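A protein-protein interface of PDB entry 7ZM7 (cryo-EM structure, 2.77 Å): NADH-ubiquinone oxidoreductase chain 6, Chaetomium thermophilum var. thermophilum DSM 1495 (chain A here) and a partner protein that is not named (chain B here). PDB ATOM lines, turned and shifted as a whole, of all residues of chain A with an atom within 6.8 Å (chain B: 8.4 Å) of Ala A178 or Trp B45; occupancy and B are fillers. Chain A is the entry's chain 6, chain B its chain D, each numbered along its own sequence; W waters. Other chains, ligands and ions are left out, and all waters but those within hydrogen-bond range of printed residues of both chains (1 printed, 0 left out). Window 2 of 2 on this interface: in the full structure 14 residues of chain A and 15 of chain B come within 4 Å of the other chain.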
ATOM      1  N   ILE A 174       7.803 -20.371   8.842  1.00  0.00           N
ATOM      2  CA  ILE A 174       6.585 -21.006   8.249  1.00  0.00           C
ATOM      3  C   ILE A 174       6.505 -22.388   8.898  1.00  0.00           C
ATOM      4  O   ILE A 174       7.549 -22.880   9.330  1.00  0.00           O
ATOM      5  CB  ILE A 174       6.699 -21.108   6.714  1.00  0.00           C
ATOM      6  CG1 ILE A 174       5.356 -21.362   6.031  1.00  0.00           C
ATOM      7  CG2 ILE A 174       7.742 -22.135   6.298  1.00  0.00           C
ATOM      8  CD1 ILE A 174       5.484 -21.667   4.560  1.00  0.00           C
ATOM      9  N   TRP A 175       5.314 -22.965   9.017  1.00  0.00           N
ATOM     10  CA  TRP A 175       5.190 -24.256   9.735  1.00  0.00           C
ATOM     11  C   TRP A 175       4.734 -25.364   8.791  1.00  0.00           C
ATOM     12  O   TRP A 175       5.311 -26.454   8.842  1.00  0.00           O
ATOM     13  CB  TRP A 175       4.272 -24.083  10.942  1.00  0.00           C
ATOM     14  CG  TRP A 175       4.847 -23.166  11.977  1.00  0.00           C
ATOM     15  CD1 TRP A 175       4.537 -21.854  12.179  1.00  0.00           C
ATOM     16  CD2 TRP A 175       5.866 -23.489  12.939  1.00  0.00           C
ATOM     17  NE1 TRP A 175       5.274 -21.345  13.212  1.00  0.00           N
ATOM     18  CE2 TRP A 175       6.100 -22.323  13.696  1.00  0.00           C
ATOM     19  CE3 TRP A 175       6.594 -24.645  13.237  1.00  0.00           C
ATOM     20  CZ2 TRP A 175       7.029 -22.285  14.733  1.00  0.00           C
ATOM     21  CZ3 TRP A 175       7.509 -24.608  14.262  1.00  0.00           C
ATOM     22  CH2 TRP A 175       7.719 -23.445  15.000  1.00  0.00           C
ATOM     23  N   ASP A 176       3.757 -25.081   7.941  1.00  0.00           N
ATOM     24  CA  ASP A 176       3.269 -26.070   6.943  1.00  0.00           C
ATOM     25  C   ASP A 176       4.397 -26.429   5.971  1.00  0.00           C
ATOM     26  O   ASP A 176       4.469 -27.606   5.579  1.00  0.00           O
ATOM     27  CB  ASP A 176       1.956 -25.629   6.284  1.00  0.00           C
ATOM     28  CG  ASP A 176       1.864 -24.162   5.900  1.00  0.00           C
ATOM     29  OD1 ASP A 176       2.918 -23.522   5.751  1.00  0.00           O
ATOM     30  OD2 ASP A 176       0.727 -23.676   5.743  1.00  0.00           O
ATOM     31  N   GLY A 177       5.236 -25.459   5.603  1.00  0.00           N
ATOM     32  CA  GLY A 177       6.357 -25.685   4.673  1.00  0.00           C
ATOM     33  C   GLY A 177       7.621 -26.182   5.352  1.00  0.00           C
ATOM     34  O   GLY A 177       8.602 -26.422   4.639  1.00  0.00           O
ATOM     35  N   ALA A 178       7.614 -26.324   6.678  1.00  0.00           N
ATOM     36  CA  ALA A 178       8.797 -26.796   7.435  1.00  0.00           C
ATOM     37  C   ALA A 178       8.549 -28.177   8.042  1.00  0.00           C
ATOM     38  O   ALA A 178       9.305 -28.545   8.931  1.00  0.00           O
ATOM     39  CB  ALA A 178       9.143 -25.796   8.508  1.00  0.00           C
ATOM     40  N   LEU A 179       7.541 -28.913   7.577  1.00  0.00           N
ATOM     41  CA  LEU A 179       7.179 -30.239   8.165  1.00  0.00           C
ATOM     42  C   LEU A 179       8.334 -31.229   7.999  1.00  0.00           C
ATOM     43  O   LEU A 179       8.817 -31.743   9.014  1.00  0.00           O
ATOM     44  CB  LEU A 179       5.912 -30.785   7.507  1.00  0.00           C
ATOM     45  CG  LEU A 179       5.559 -32.235   7.844  1.00  0.00           C
ATOM     46  CD1 LEU A 179       5.077 -32.366   9.277  1.00  0.00           C
ATOM     47  CD2 LEU A 179       4.515 -32.783   6.889  1.00  0.00           C
ATOM     48  N   ALA A 180       8.772 -31.449   6.762  1.00  0.00           N
ATOM     49  CA  ALA A 180       9.894 -32.369   6.500  1.00  0.00           C
ATOM     50  C   ALA A 180      10.867 -31.696   5.535  1.00  0.00           C
ATOM     51  O   ALA A 180      10.946 -32.121   4.387  1.00  0.00           O
ATOM     52  CB  ALA A 180       9.362 -33.666   5.964  1.00  0.00           C
ATOM     53  N   GLU A 181      11.603 -30.695   6.000  1.00  0.00           N
ATOM     54  CA  GLU A 181      12.531 -29.934   5.129  1.00  0.00           C
ATOM     55  C   GLU A 181      13.652 -30.832   4.611  1.00  0.00           C
ATOM     56  O   GLU A 181      14.110 -31.724   5.350  1.00  0.00           O
ATOM     57  CB  GLU A 181      13.074 -28.702   5.849  1.00  0.00           C
ATOM     58  CG  GLU A 181      14.058 -27.872   5.050  1.00  0.00           C
ATOM     59  CD  GLU A 181      15.478 -27.866   5.590  1.00  0.00           C
ATOM     60  OE1 GLU A 181      16.269 -27.011   5.147  1.00  0.00           O
ATOM     61  OE2 GLU A 181      15.792 -28.718   6.447  1.00  0.00           O
ATOM     62  N   ARG B  39      20.577 -30.587  21.817  1.00  0.00           N
ATOM     63  CA  ARG B  39      19.822 -31.074  20.636  1.00  0.00           C
ATOM     64  C   ARG B  39      20.817 -31.521  19.562  1.00  0.00           C
ATOM     65  O   ARG B  39      21.897 -30.938  19.497  1.00  0.00           O
ATOM     66  CB  ARG B  39      18.886 -29.963  20.154  1.00  0.00           C
ATOM     67  CG  ARG B  39      17.782 -29.609  21.136  1.00  0.00           C
ATOM     68  CD  ARG B  39      16.808 -30.756  21.268  1.00  0.00           C
ATOM     69  NE  ARG B  39      16.202 -31.040  19.979  1.00  0.00           N
ATOM     70  CZ  ARG B  39      14.983 -30.667  19.625  1.00  0.00           C
ATOM     71  NH1 ARG B  39      14.221 -30.014  20.482  1.00  0.00           N
ATOM     72  NH2 ARG B  39      14.518 -30.966  18.428  1.00  0.00           N
ATOM     73  N   SER B  41      20.149 -33.563  15.598  1.00  0.00           N
ATOM     74  CA  SER B  41      19.868 -33.409  14.143  1.00  0.00           C
ATOM     75  C   SER B  41      18.769 -32.370  13.912  1.00  0.00           C
ATOM     76  O   SER B  41      17.667 -32.751  13.502  1.00  0.00           O
ATOM     77  CB  SER B  41      19.544 -34.745  13.532  1.00  0.00           C
ATOM     78  OG  SER B  41      20.638 -35.637  13.675  1.00  0.00           O
ATOM     79  N   VAL B  42      19.079 -31.095  14.131  1.00  0.00           N
ATOM     80  CA  VAL B  42      18.035 -30.032  14.131  1.00  0.00           C
ATOM     81  C   VAL B  42      17.726 -29.477  12.739  1.00  0.00           C
ATOM     82  O   VAL B  42      18.637 -28.944  12.090  1.00  0.00           O
ATOM     83  CB  VAL B  42      18.419 -28.926  15.133  1.00  0.00           C
ATOM     84  CG1 VAL B  42      18.270 -29.406  16.566  1.00  0.00           C
ATOM     85  CG2 VAL B  42      19.825 -28.398  14.902  1.00  0.00           C
ATOM     86  N   ASP B  43      16.475 -29.609  12.301  1.00  0.00           N
ATOM     87  CA  ASP B  43      16.027 -29.055  11.004  1.00  0.00           C
ATOM     88  C   ASP B  43      15.399 -27.674  11.210  1.00  0.00           C
ATOM     89  O   ASP B  43      15.410 -27.196  12.341  1.00  0.00           O
ATOM     90  CB  ASP B  43      15.064 -30.018  10.314  1.00  0.00           C
ATOM     91  CG  ASP B  43      13.959 -30.562  11.205  1.00  0.00           C
ATOM     92  OD1 ASP B  43      13.459 -29.811  12.053  1.00  0.00           O
ATOM     93  OD2 ASP B  43      13.604 -31.740  11.034  1.00  0.00           O
ATOM     94  N   GLN B  44      14.798 -27.113  10.157  1.00  0.00           N
ATOM     95  CA  GLN B  44      14.160 -25.778  10.214  1.00  0.00           C
ATOM     96  C   GLN B  44      13.052 -25.789  11.264  1.00  0.00           C
ATOM     97  O   GLN B  44      12.950 -24.809  11.999  1.00  0.00           O
ATOM     98  CB  GLN B  44      13.570 -25.481   8.837  1.00  0.00           C
ATOM     99  CG  GLN B  44      12.986 -24.085   8.701  1.00  0.00           C
ATOM    100  CD  GLN B  44      12.089 -23.985   7.493  1.00  0.00           C
ATOM    101  OE1 GLN B  44      11.948 -24.932   6.723  1.00  0.00           O
ATOM    102  NE2 GLN B  44      11.466 -22.831   7.322  1.00  0.00           N
ATOM    103  N   TRP B  45      12.276 -26.867  11.332  1.00  0.00           N
ATOM    104  CA  TRP B  45      11.185 -26.973  12.330  1.00  0.00           C
ATOM    105  C   TRP B  45      11.734 -26.913  13.753  1.00  0.00           C
ATOM    106  O   TRP B  45      11.198 -26.131  14.537  1.00  0.00           O
ATOM    107  CB  TRP B  45      10.438 -28.291  12.123  1.00  0.00           C
ATOM    108  CG  TRP B  45       9.351 -28.571  13.113  1.00  0.00           C
ATOM    109  CD1 TRP B  45       9.487 -29.000  14.401  1.00  0.00           C
ATOM    110  CD2 TRP B  45       7.938 -28.467  12.876  1.00  0.00           C
ATOM    111  NE1 TRP B  45       8.261 -29.148  14.987  1.00  0.00           N
ATOM    112  CE2 TRP B  45       7.291 -28.829  14.076  1.00  0.00           C
ATOM    113  CE3 TRP B  45       7.162 -28.096  11.774  1.00  0.00           C
ATOM    114  CZ2 TRP B  45       5.905 -28.829  14.201  1.00  0.00           C
ATOM    115  CZ3 TRP B  45       5.793 -28.094  11.901  1.00  0.00           C
ATOM    116  CH2 TRP B  45       5.176 -28.454  13.098  1.00  0.00           C
ATOM    117  N   ASP B  46      12.785 -27.667  14.050  1.00  0.00           N
ATOM    118  CA  ASP B  46      13.318 -27.747  15.433  1.00  0.00           C
ATOM    119  C   ASP B  46      13.881 -26.389  15.832  1.00  0.00           C
ATOM    120  O   ASP B  46      13.688 -25.983  16.982  1.00  0.00           O
ATOM    121  CB  ASP B  46      14.397 -28.827  15.527  1.00  0.00           C
ATOM    122  CG  ASP B  46      13.915 -30.211  15.142  1.00  0.00           C
ATOM    123  OD1 ASP B  46      12.722 -30.491  15.345  1.00  0.00           O
ATOM    124  OD2 ASP B  46      14.738 -30.995  14.635  1.00  0.00           O
ATOM    125  N   LYS B  47      14.561 -25.728  14.904  1.00  0.00           N
ATOM    126  CA  LYS B  47      15.160 -24.393  15.178  1.00  0.00           C
ATOM    127  C   LYS B  47      14.083 -23.345  15.449  1.00  0.00           C
ATOM    128  O   LYS B  47      14.248 -22.574  16.382  1.00  0.00           O
ATOM    129  CB  LYS B  47      16.009 -23.988  13.976  1.00  0.00           C
ATOM    130  CG  LYS B  47      17.223 -24.869  13.715  1.00  0.00           C
ATOM    131  CD  LYS B  47      17.902 -24.558  12.403  1.00  0.00           C
ATOM    132  CE  LYS B  47      18.867 -25.637  11.966  1.00  0.00           C
ATOM    133  NZ  LYS B  47      19.493 -25.320  10.660  1.00  0.00           N
ATOM    134  N   GLN B  48      13.024 -23.330  14.653  1.00  0.00           N
ATOM    135  CA  GLN B  48      11.902 -22.401  14.877  1.00  0.00           C
ATOM    136  C   GLN B  48      11.215 -22.742  16.195  1.00  0.00           C
ATOM    137  O   GLN B  48      10.797 -21.810  16.891  1.00  0.00           O
ATOM    138  CB  GLN B  48      10.945 -22.483  13.694  1.00  0.00           C
ATOM    139  CG  GLN B  48      11.561 -22.021  12.385  1.00  0.00           C
ATOM    140  CD  GLN B  48      10.621 -22.253  11.234  1.00  0.00           C
ATOM    141  OE1 GLN B  48      10.827 -21.757  10.132  1.00  0.00           O
ATOM    142  NE2 GLN B  48       9.570 -23.010  11.489  1.00  0.00           N
ATOM    143  N   GLN B  49      11.089 -24.027  16.511  1.00  0.00           N
ATOM    144  CA  GLN B  49      10.463 -24.443  17.787  1.00  0.00           C
ATOM    145  C   GLN B  49      11.279 -23.892  18.957  1.00  0.00           C
ATOM    146  O   GLN B  49      10.670 -23.389  19.907  1.00  0.00           O
ATOM    147  CB  GLN B  49      10.252 -25.956  17.808  1.00  0.00           C
ATOM    148  CG  GLN B  49       9.002 -26.416  17.077  1.00  0.00           C
ATOM    149  CD  GLN B  49       7.742 -26.114  17.848  1.00  0.00           C
ATOM    150  OE1 GLN B  49       7.749 -25.358  18.813  1.00  0.00           O
ATOM    151  NE2 GLN B  49       6.642 -26.712  17.430  1.00  0.00           N
ATOM    152  N   MET B  50      12.600 -23.953  18.876  1.00  0.00           N
ATOM    153  CA  MET B  50      13.483 -23.355  19.909  1.00  0.00           C
ATOM    154  C   MET B  50      13.346 -21.829  19.929  1.00  0.00           C
ATOM    155  O   MET B  50      13.440 -21.257  21.014  1.00  0.00           O
ATOM    156  CB  MET B  50      14.935 -23.754  19.682  1.00  0.00           C
ATOM    157  CG  MET B  50      15.254 -25.136  20.205  1.00  0.00           C
ATOM    158  SD  MET B  50      17.005 -25.547  20.071  1.00  0.00           S
ATOM    159  CE  MET B  50      17.138 -25.831  18.309  1.00  0.00           C
ATOM    160  N   GLU B  51      13.166 -21.193  18.779  1.00  0.00           N
ATOM    161  CA  GLU B  51      12.946 -19.728  18.724  1.00  0.00           C
ATOM    162  C   GLU B  51      11.665 -19.342  19.470  1.00  0.00           C
ATOM    163  O   GLU B  51      11.645 -18.268  20.063  1.00  0.00           O
ATOM    164  CB  GLU B  51      13.055 -19.230  17.286  1.00  0.00           C
ATOM    165  CG  GLU B  51      14.490 -19.000  16.874  1.00  0.00           C
ATOM    166  CD  GLU B  51      14.680 -18.336  15.526  1.00  0.00           C
ATOM    167  OE1 GLU B  51      13.722 -17.715  15.031  1.00  0.00           O
ATOM    168  OE2 GLU B  51      15.787 -18.460  14.973  1.00  0.00           O
ATOM    169  N   ARG B  52      10.638 -20.180  19.418  1.00  0.00           N
ATOM    170  CA  ARG B  52       9.352 -19.849  20.067  1.00  0.00           C
ATOM    171  C   ARG B  52       9.536 -20.195  21.533  1.00  0.00           C
ATOM    172  O   ARG B  52       8.836 -19.610  22.365  1.00  0.00           O
ATOM    173  CB  ARG B  52       8.208 -20.607  19.397  1.00  0.00           C
ATOM    174  CG  ARG B  52       6.839 -20.382  20.019  1.00  0.00           C
ATOM    175  CD  ARG B  52       5.825 -21.327  19.416  1.00  0.00           C
ATOM    176  NE  ARG B  52       4.482 -20.982  19.840  1.00  0.00           N
ATOM    177  CZ  ARG B  52       3.784 -21.657  20.739  1.00  0.00           C
ATOM    178  NH1 ARG B  52       4.298 -22.737  21.299  1.00  0.00           N
ATOM    179  NH2 ARG B  52       2.567 -21.259  21.060  1.00  0.00           N
HETATM  180  O   HOH W   1      11.757 -29.101   8.874  1.00  0.00           O
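NE2 of Gln B48 sits at hydrogen-bond distance from O of Ile A174, 3.0 Å away.
OD1 of Asp B43 sits close to N of Trp B45 (3.3 Å). The side-chain amide oxygen (OE1) of Gln B48 is in hydrogen-bond range of the side-chain amide nitrogen (NE2) of Gln B44 (3.1 Å).
Among the printed residues, pairs that only touch across the chains: Ile A174 with Gln B44, Trp A175 with Trp B45, Trp A175 with Gln B48, Trp A175 with Gln B49, Ala A178 with Gln B44, Ala A178 with Trp B45 and Glu A181 with Gln B44.
Of the printed residues of chain B, Trp A175 touches Trp B45, Gln B48 and Gln B49. Gly A177 touches none of the printed residues of chain B. Ala A178 touches just these residues of chain B: Gln B44 (3.4 Å) and Trp B45 (3.4 Å). Printed residues of chain B within 4 Å of Glu A181: Gln B44 (3.99 Å). Of the printed residues of chain A, Gln B44 touches Ile A174 (3.9 Å), Ala A178 (3.4 Å) and Glu A181 (3.99 Å). Trp B45 touches just these residues of chain A: Trp A175 and Ala A178. Of the printed residues of chain A, Gln B49 touches Trp A175 (3.7 Å). Arg B52 touches none of the printed residues of chain A. The nearest residue of chain B that does not touch Ala A178 is Gln B48 (4.1 Å). The nearest residue of chain A that does not touch Trp B45 is Leu A179 (4.2 Å). The nearest printed residue of chain A that does not touch Gln B44 is Gly A177 (4.2 Å).
Printed residues of chain A that touch a printed residue of chain B: Ile A174, Trp A175, Ala A178 and Glu A181. Among the printed residues, no Asp or Glu carboxylate lies within 4 Å of a Lys or Arg side-chain nitrogen of the other chain.
Water W1 lies within hydrogen-bond range of O of Ala A178 (2.5 Å), N of Glu A181 (3.3 Å) and N of Trp B45 (3.4 Å).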
